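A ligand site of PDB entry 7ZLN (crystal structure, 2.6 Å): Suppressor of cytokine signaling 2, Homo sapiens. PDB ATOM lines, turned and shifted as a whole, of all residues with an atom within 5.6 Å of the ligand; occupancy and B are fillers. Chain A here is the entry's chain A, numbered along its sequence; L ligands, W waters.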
ATOM      1  N   MET A  24      24.405  32.436  -4.828  1.00  0.00           N
ATOM      2  CA  MET A  24      25.201  31.215  -4.788  1.00  0.00           C
ATOM      3  C   MET A  24      24.853  30.391  -6.023  1.00  0.00           C
ATOM      4  O   MET A  24      23.715  30.417  -6.497  1.00  0.00           O
ATOM      5  CB  MET A  24      24.928  30.414  -3.518  1.00  0.00           C
ATOM      6  CG  MET A  24      26.012  29.422  -3.126  1.00  0.00           C
ATOM      7  SD  MET A  24      25.676  28.724  -1.497  1.00  0.00           S
ATOM      8  CE  MET A  24      26.975  27.507  -1.352  1.00  0.00           C
ATOM      9  N   VAL A  26      24.855  26.585  -8.217  1.00  0.00           N
ATOM     10  CA  VAL A  26      24.602  25.167  -7.955  1.00  0.00           C
ATOM     11  C   VAL A  26      25.910  24.449  -7.660  1.00  0.00           C
ATOM     12  O   VAL A  26      25.984  23.612  -6.747  1.00  0.00           O
ATOM     13  CB  VAL A  26      23.874  24.533  -9.154  1.00  0.00           C
ATOM     14  CG1 VAL A  26      22.393  24.791  -9.052  1.00  0.00           C
ATOM     15  CG2 VAL A  26      24.420  25.079 -10.464  1.00  0.00           C
ATOM     16  N   ASN A  27      26.960  24.768  -8.420  1.00  0.00           N
ATOM     17  CA  ASN A  27      28.250  24.105  -8.215  1.00  0.00           C
ATOM     18  C   ASN A  27      28.885  24.537  -6.893  1.00  0.00           C
ATOM     19  O   ASN A  27      29.516  23.728  -6.211  1.00  0.00           O
ATOM     20  CB  ASN A  27      29.168  24.413  -9.393  1.00  0.00           C
ATOM     21  CG  ASN A  27      28.543  24.057 -10.722  1.00  0.00           C
ATOM     22  OD1 ASN A  27      28.115  22.925 -10.941  1.00  0.00           O
ATOM     23  ND2 ASN A  27      28.472  25.041 -11.619  1.00  0.00           N
ATOM     24  N   LYS A  30      26.732  22.478  -4.494  1.00  0.00           N
ATOM     25  CA  LYS A  30      27.142  21.080  -4.522  1.00  0.00           C
ATOM     26  C   LYS A  30      28.427  20.857  -3.727  1.00  0.00           C
ATOM     27  O   LYS A  30      28.587  19.833  -3.053  1.00  0.00           O
ATOM     28  CB  LYS A  30      27.311  20.617  -5.970  1.00  0.00           C
ATOM     29  CG  LYS A  30      28.052  19.310  -6.140  1.00  0.00           C
ATOM     30  CD  LYS A  30      28.528  19.157  -7.574  1.00  0.00           C
ATOM     31  CE  LYS A  30      29.554  20.235  -7.926  1.00  0.00           C
ATOM     32  NZ  LYS A  30      29.991  20.138  -9.352  1.00  0.00           N
ATOM     33  N   ARG A  44      19.315  29.749  -1.209  1.00  0.00           N
ATOM     34  CA  ARG A  44      20.094  30.698  -1.985  1.00  0.00           C
ATOM     35  C   ARG A  44      19.218  31.239  -3.106  1.00  0.00           C
ATOM     36  O   ARG A  44      18.150  30.711  -3.412  1.00  0.00           O
ATOM     37  CB  ARG A  44      21.345  30.030  -2.570  1.00  0.00           C
ATOM     38  CG  ARG A  44      21.069  28.664  -3.174  1.00  0.00           C
ATOM     39  CD  ARG A  44      22.157  28.219  -4.130  1.00  0.00           C
ATOM     40  NE  ARG A  44      21.836  26.935  -4.725  1.00  0.00           N
ATOM     41  CZ  ARG A  44      21.237  26.768  -5.893  1.00  0.00           C
ATOM     42  NH1 ARG A  44      20.921  27.809  -6.653  1.00  0.00           N
ATOM     43  NH2 ARG A  44      20.931  25.538  -6.304  1.00  0.00           N
ATOM     44  N   ASP A  45      19.691  32.325  -3.730  1.00  0.00           N
ATOM     45  CA  ASP A  45      19.004  32.866  -4.891  1.00  0.00           C
ATOM     46  C   ASP A  45      19.042  31.860  -6.041  1.00  0.00           C
ATOM     47  O   ASP A  45      19.937  31.011  -6.127  1.00  0.00           O
ATOM     48  CB  ASP A  45      19.634  34.190  -5.317  1.00  0.00           C
ATOM     49  CG  ASP A  45      19.581  35.244  -4.217  1.00  0.00           C
ATOM     50  OD1 ASP A  45      18.799  35.076  -3.261  1.00  0.00           O
ATOM     51  OD2 ASP A  45      20.332  36.246  -4.310  1.00  0.00           O
ATOM     52  N   SER A  46      18.056  31.967  -6.929  1.00  0.00           N
ATOM     53  CA  SER A  46      17.900  31.032  -8.027  1.00  0.00           C
ATOM     54  C   SER A  46      18.454  31.617  -9.314  1.00  0.00           C
ATOM     55  O   SER A  46      18.372  32.820  -9.560  1.00  0.00           O
ATOM     56  CB  SER A  46      16.432  30.651  -8.209  1.00  0.00           C
ATOM     57  OG  SER A  46      16.243  29.906  -9.405  1.00  0.00           O
ATOM     58  N   SER A  47      19.024  30.738 -10.141  1.00  0.00           N
ATOM     59  CA  SER A  47      19.571  31.108 -11.437  1.00  0.00           C
ATOM     60  C   SER A  47      18.538  30.999 -12.559  1.00  0.00           C
ATOM     61  O   SER A  47      18.930  30.961 -13.736  1.00  0.00           O
ATOM     62  CB  SER A  47      20.796  30.256 -11.759  1.00  0.00           C
ATOM     63  OG  SER A  47      21.558  29.983 -10.590  1.00  0.00           O
ATOM     64  N   HIS A  48      17.253  30.949 -12.236  1.00  0.00           N
ATOM     65  CA  HIS A  48      16.193  30.912 -13.227  1.00  0.00           C
ATOM     66  C   HIS A  48      15.418  32.219 -13.202  1.00  0.00           C
ATOM     67  O   HIS A  48      15.220  32.816 -12.134  1.00  0.00           O
ATOM     68  CB  HIS A  48      15.236  29.736 -12.982  1.00  0.00           C
ATOM     69  CG  HIS A  48      14.461  29.338 -14.197  1.00  0.00           C
ATOM     70  ND1 HIS A  48      13.269  29.927 -14.555  1.00  0.00           N
ATOM     71  CD2 HIS A  48      14.722  28.405 -15.150  1.00  0.00           C
ATOM     72  CE1 HIS A  48      12.826  29.377 -15.670  1.00  0.00           C
ATOM     73  NE2 HIS A  48      13.689  28.448 -16.055  1.00  0.00           N
ATOM     74  N   LEU A  53      14.280  32.168  -5.053  1.00  0.00           N
ATOM     75  CA  LEU A  53      15.082  31.367  -4.141  1.00  0.00           C
ATOM     76  C   LEU A  53      15.038  29.893  -4.533  1.00  0.00           C
ATOM     77  O   LEU A  53      14.188  29.450  -5.305  1.00  0.00           O
ATOM     78  CB  LEU A  53      14.606  31.542  -2.696  1.00  0.00           C
ATOM     79  CG  LEU A  53      14.674  32.977  -2.173  1.00  0.00           C
ATOM     80  CD1 LEU A  53      13.688  33.185  -1.033  1.00  0.00           C
ATOM     81  CD2 LEU A  53      16.093  33.314  -1.726  1.00  0.00           C
ATOM     82  N   THR A  54      15.983  29.126  -3.976  1.00  0.00           N
ATOM     83  CA  THR A  54      16.134  27.719  -4.294  1.00  0.00           C
ATOM     84  C   THR A  54      16.735  26.993  -3.099  1.00  0.00           C
ATOM     85  O   THR A  54      17.672  27.483  -2.476  1.00  0.00           O
ATOM     86  CB  THR A  54      17.019  27.522  -5.535  1.00  0.00           C
ATOM     87  OG1 THR A  54      16.266  27.847  -6.711  1.00  0.00           O
ATOM     88  CG2 THR A  54      17.520  26.090  -5.634  1.00  0.00           C
ATOM     89  N   VAL A  57      19.921  20.856  -0.900  1.00  0.00           N
ATOM     90  CA  VAL A  57      19.832  19.886   0.192  1.00  0.00           C
ATOM     91  C   VAL A  57      20.651  18.645  -0.168  1.00  0.00           C
ATOM     92  O   VAL A  57      20.719  18.248  -1.333  1.00  0.00           O
ATOM     93  CB  VAL A  57      18.364  19.516   0.493  1.00  0.00           C
ATOM     94  CG1 VAL A  57      17.694  18.897  -0.729  1.00  0.00           C
ATOM     95  CG2 VAL A  57      18.266  18.586   1.696  1.00  0.00           C
ATOM     96  N   PRO A  63      24.326  16.139  -3.167  1.00  0.00           N
ATOM     97  CA  PRO A  63      23.544  17.378  -3.114  1.00  0.00           C
ATOM     98  C   PRO A  63      22.605  17.500  -4.308  1.00  0.00           C
ATOM     99  O   PRO A  63      22.966  17.174  -5.439  1.00  0.00           O
ATOM    100  CB  PRO A  63      24.604  18.485  -3.140  1.00  0.00           C
ATOM    101  CG  PRO A  63      25.879  17.809  -2.716  1.00  0.00           C
ATOM    102  CD  PRO A  63      25.767  16.413  -3.263  1.00  0.00           C
ATOM    103  N   THR A  64      21.388  17.960  -4.040  1.00  0.00           N
ATOM    104  CA  THR A  64      20.396  18.256  -5.061  1.00  0.00           C
ATOM    105  C   THR A  64      19.786  19.627  -4.764  1.00  0.00           C
ATOM    106  O   THR A  64      20.116  20.265  -3.769  1.00  0.00           O
ATOM    107  CB  THR A  64      19.310  17.172  -5.118  1.00  0.00           C
ATOM    108  OG1 THR A  64      18.302  17.551  -6.068  1.00  0.00           O
ATOM    109  CG2 THR A  64      18.668  16.987  -3.755  1.00  0.00           C
ATOM    110  N   ASN A  65      18.892  20.074  -5.649  1.00  0.00           N
ATOM    111  CA  ASN A  65      18.377  21.435  -5.574  1.00  0.00           C
ATOM    112  C   ASN A  65      16.894  21.447  -5.904  1.00  0.00           C
ATOM    113  O   ASN A  65      16.457  20.809  -6.871  1.00  0.00           O
ATOM    114  CB  ASN A  65      19.134  22.359  -6.545  1.00  0.00           C
ATOM    115  CG  ASN A  65      20.621  22.080  -6.576  1.00  0.00           C
ATOM    116  OD1 ASN A  65      21.387  22.639  -5.789  1.00  0.00           O
ATOM    117  ND2 ASN A  65      21.044  21.198  -7.469  1.00  0.00           N
ATOM    118  N   LEU A  66      16.118  22.169  -5.096  1.00  0.00           N
ATOM    119  CA  LEU A  66      14.703  22.389  -5.351  1.00  0.00           C
ATOM    120  C   LEU A  66      14.408  23.884  -5.327  1.00  0.00           C
ATOM    121  O   LEU A  66      14.861  24.600  -4.426  1.00  0.00           O
ATOM    122  CB  LEU A  66      13.818  21.673  -4.335  1.00  0.00           C
ATOM    123  CG  LEU A  66      12.382  21.479  -4.839  1.00  0.00           C
ATOM    124  CD1 LEU A  66      12.292  20.268  -5.749  1.00  0.00           C
ATOM    125  CD2 LEU A  66      11.405  21.366  -3.671  1.00  0.00           C
ATOM    126  N   ARG A  67      13.648  24.345  -6.318  1.00  0.00           N
ATOM    127  CA  ARG A  67      13.289  25.751  -6.425  1.00  0.00           C
ATOM    128  C   ARG A  67      12.008  26.035  -5.647  1.00  0.00           C
ATOM    129  O   ARG A  67      11.157  25.152  -5.469  1.00  0.00           O
ATOM    130  CB  ARG A  67      13.112  26.147  -7.889  1.00  0.00           C
ATOM    131  CG  ARG A  67      14.396  26.083  -8.699  1.00  0.00           C
ATOM    132  CD  ARG A  67      14.149  26.357 -10.165  1.00  0.00           C
ATOM    133  NE  ARG A  67      15.395  26.437 -10.913  1.00  0.00           N
ATOM    134  CZ  ARG A  67      15.583  25.904 -12.110  1.00  0.00           C
ATOM    135  NH1 ARG A  67      14.618  25.245 -12.732  1.00  0.00           N
ATOM    136  NH2 ARG A  67      16.767  26.038 -12.702  1.00  0.00           N
ATOM    137  N   ILE A  81       6.933  19.524  -9.736  1.00  0.00           N
ATOM    138  CA  ILE A  81       7.197  18.206  -9.153  1.00  0.00           C
ATOM    139  C   ILE A  81       5.937  17.525  -8.660  1.00  0.00           C
ATOM    140  O   ILE A  81       5.962  16.306  -8.400  1.00  0.00           O
ATOM    141  CB  ILE A  81       8.216  18.297  -7.993  1.00  0.00           C
ATOM    142  CG1 ILE A  81       7.901  19.508  -7.096  1.00  0.00           C
ATOM    143  CG2 ILE A  81       9.630  18.420  -8.520  1.00  0.00           C
ATOM    144  CD1 ILE A  81       8.516  19.436  -5.704  1.00  0.00           C
ATOM    145  N   HIS A 120       8.126  14.733  -1.452  1.00  0.00           N
ATOM    146  CA  HIS A 120       9.093  14.116  -0.555  1.00  0.00           C
ATOM    147  C   HIS A 120      10.292  15.047  -0.412  1.00  0.00           C
ATOM    148  O   HIS A 120      11.079  15.187  -1.348  1.00  0.00           O
ATOM    149  CB  HIS A 120       9.538  12.746  -1.072  1.00  0.00           C
ATOM    150  CG  HIS A 120      10.732  12.192  -0.370  1.00  0.00           C
ATOM    151  ND1 HIS A 120      10.848  12.197   1.012  1.00  0.00           N
ATOM    152  CD2 HIS A 120      11.871  11.646  -0.841  1.00  0.00           C
ATOM    153  CE1 HIS A 120      12.001  11.657   1.348  1.00  0.00           C
ATOM    154  NE2 HIS A 120      12.645  11.305   0.247  1.00  0.00           N
ATOM    155  N   LEU A 121      10.423  15.667   0.753  1.00  0.00           N
ATOM    156  CA  LEU A 121      11.532  16.565   1.046  1.00  0.00           C
ATOM    157  C   LEU A 121      12.082  16.219   2.421  1.00  0.00           C
ATOM    158  O   LEU A 121      11.398  16.429   3.432  1.00  0.00           O
ATOM    159  CB  LEU A 121      11.101  18.031   0.974  1.00  0.00           C
ATOM    160  CG  LEU A 121      12.214  19.073   0.841  1.00  0.00           C
ATOM    161  CD1 LEU A 121      13.261  18.632  -0.160  1.00  0.00           C
ATOM    162  CD2 LEU A 121      11.629  20.427   0.455  1.00  0.00           C
HETATM  163  C1  LIG L   1      22.729  20.030 -10.652  1.00  0.00           C
HETATM  164  C2  LIG L   1      16.324  18.667 -10.034  1.00  0.00           C
HETATM  165  C3  LIG L   1      14.407  17.575  -8.842  1.00  0.00           C
HETATM  166  C4  LIG L   1      12.542  16.992  -7.263  1.00  0.00           C
HETATM  167  C5  LIG L   1      14.176  17.321  -5.052  1.00  0.00           C
HETATM  168  C6  LIG L   1      15.072  17.510  -3.831  1.00  0.00           C
HETATM  169  C7  LIG L   1      17.626  22.209 -10.487  1.00  0.00           C
HETATM  170  C8  LIG L   1      17.494  24.251  -9.218  1.00  0.00           C
HETATM  171  C9  LIG L   1      19.751  18.830  -9.840  1.00  0.00           C
HETATM  172  C10 LIG L   1      21.013  18.202 -10.422  1.00  0.00           C
HETATM  173  C11 LIG L   1      22.254  18.937  -9.939  1.00  0.00           C
HETATM  174  C12 LIG L   1      22.901  18.524  -8.787  1.00  0.00           C
HETATM  175  C13 LIG L   1      24.030  19.199  -8.349  1.00  0.00           C
HETATM  176  C14 LIG L   1      24.505  20.293  -9.062  1.00  0.00           C
HETATM  177  C15 LIG L   1      23.859  20.706 -10.214  1.00  0.00           C
HETATM  178  C16 LIG L   1      17.427  19.720 -10.108  1.00  0.00           C
HETATM  179  C17 LIG L   1      13.870  17.360  -7.428  1.00  0.00           C
HETATM  180  C18 LIG L   1      12.027  16.792  -5.998  1.00  0.00           C
HETATM  181  C19 LIG L   1      12.853  16.962  -4.886  1.00  0.00           C
HETATM  182  C20 LIG L   1      14.684  17.527  -6.328  1.00  0.00           C
HETATM  183  C21 LIG L   1      16.986  20.912 -10.967  1.00  0.00           C
HETATM  184  C22 LIG L   1      16.916  23.065  -9.666  1.00  0.00           C
HETATM  185  C23 LIG L   1      18.788  24.567  -9.600  1.00  0.00           C
HETATM  186  C24 LIG L   1      19.499  23.711 -10.421  1.00  0.00           C
HETATM  187  C25 LIG L   1      18.919  22.525 -10.860  1.00  0.00           C
HETATM  188  F1  LIG L   1      25.618  20.957  -8.636  1.00  0.00           F
HETATM  189  F2  LIG L   1      12.352  16.765  -3.628  1.00  0.00           F
HETATM  190  N1  LIG L   1      18.614  19.123 -10.686  1.00  0.00           N
HETATM  191  N2  LIG L   1      15.449  18.590  -8.873  1.00  0.00           N
HETATM  192  O1  LIG L   1      19.712  19.096  -8.687  1.00  0.00           O
HETATM  193  O2  LIG L   1      16.184  17.911 -10.933  1.00  0.00           O
HETATM  194  O3  LIG L   1      19.371  25.762  -9.151  1.00  0.00           O
HETATM  195  O4  LIG L   1      18.320  27.097 -11.107  1.00  0.00           O
HETATM  196  O5  LIG L   1      19.907  28.240  -9.605  1.00  0.00           O
HETATM  197  O6  LIG L   1      17.658  27.640  -8.793  1.00  0.00           O
HETATM  198  P1  LIG L   1      18.807  27.210  -9.681  1.00  0.00           P
HETATM  199  O   HOH W   1      17.904  18.758 -13.776  1.00  0.00           O
HETATM  200  O   HOH W   2      18.723  15.583  -9.518  1.00  0.00           O
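OG of Ser 47 is in hydrogen-bond range of O5 of the ligand (2.6 Å).
An oxygen (O6) of the ligand lies within hydrogen-bond range of the side-chain hydroxyl (OG1) of Thr 54 (2.5 Å).
OG1 of Thr 64 sits at hydrogen-bond distance from O1 of the ligand, at 3.4 Å.
An oxygen (O5) of the ligand is in salt-bridge range of the guanidinium group (NH1) of Arg 44, at 3.2 Å.
The backbone NH of Ser 47 sits at hydrogen-bond distance from an oxygen (O5) of the ligand (2.7 Å).
The side-chain amide nitrogen (ND2) of Asn 65 lies within hydrogen-bond range of an oxygen (O1) of the ligand (2.8 Å).
The guanidinium group of Arg 67 lies within salt-bridge range of an oxygen (O4) of the ligand, at 2.5 Å.
The side-chain hydroxyl of Ser 46 sits at hydrogen-bond distance from an oxygen (O6) of the ligand, 2.7 Å away.
The backbone NH (N) of Asn 65 sits at hydrogen-bond distance from an oxygen (O1) of the ligand (3.3 Å).
N2 of the ligand is in hydrogen-bond range of O of Asn 65 (3.2 Å).
The backbone NH of Thr 54 sits at hydrogen-bond distance from the backbone carbonyl oxygen of Arg 44.
The side-chain hydroxyl (OG) of Ser 46 lies within hydrogen-bond range of the backbone NH (N) of His 48 (3.2 Å).
OG1 of Thr 54 lies close to OG of Ser 46.
The side-chain amide oxygen (OD1) of Asn 65 is in hydrogen-bond range of the guanidinium group (NH2) of Arg 44 (3.0 Å).
The backbone NH (N) of Thr 64 lies within hydrogen-bond range of the backbone carbonyl oxygen (O) of Val 57.
A fluorine (F1) of the ligand lies close to the backbone carbonyl oxygen of Val 26 (3.3 Å).
The backbone carbonyl oxygen (O) of His 120 sits close to a fluorine (F2) of the ligand, at 3.1 Å.
Asn 27 touches the ligand.
Lys 30 touches the ligand (CB to F1, 3.2 Å).
Pro 63 touches the ligand (O to C12, 3.6 Å).
CD1 of Leu 66 touches C19 of the ligand, 3.5 Å away.
CG2 of Ile 81 touches C4 of the ligand, at 3.5 Å.
Of the 20 residues printed, 14 come within 4 Å of the ligand.
The nearest printed residue that does not touch the ligand is Leu 121 (4.04 Å).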
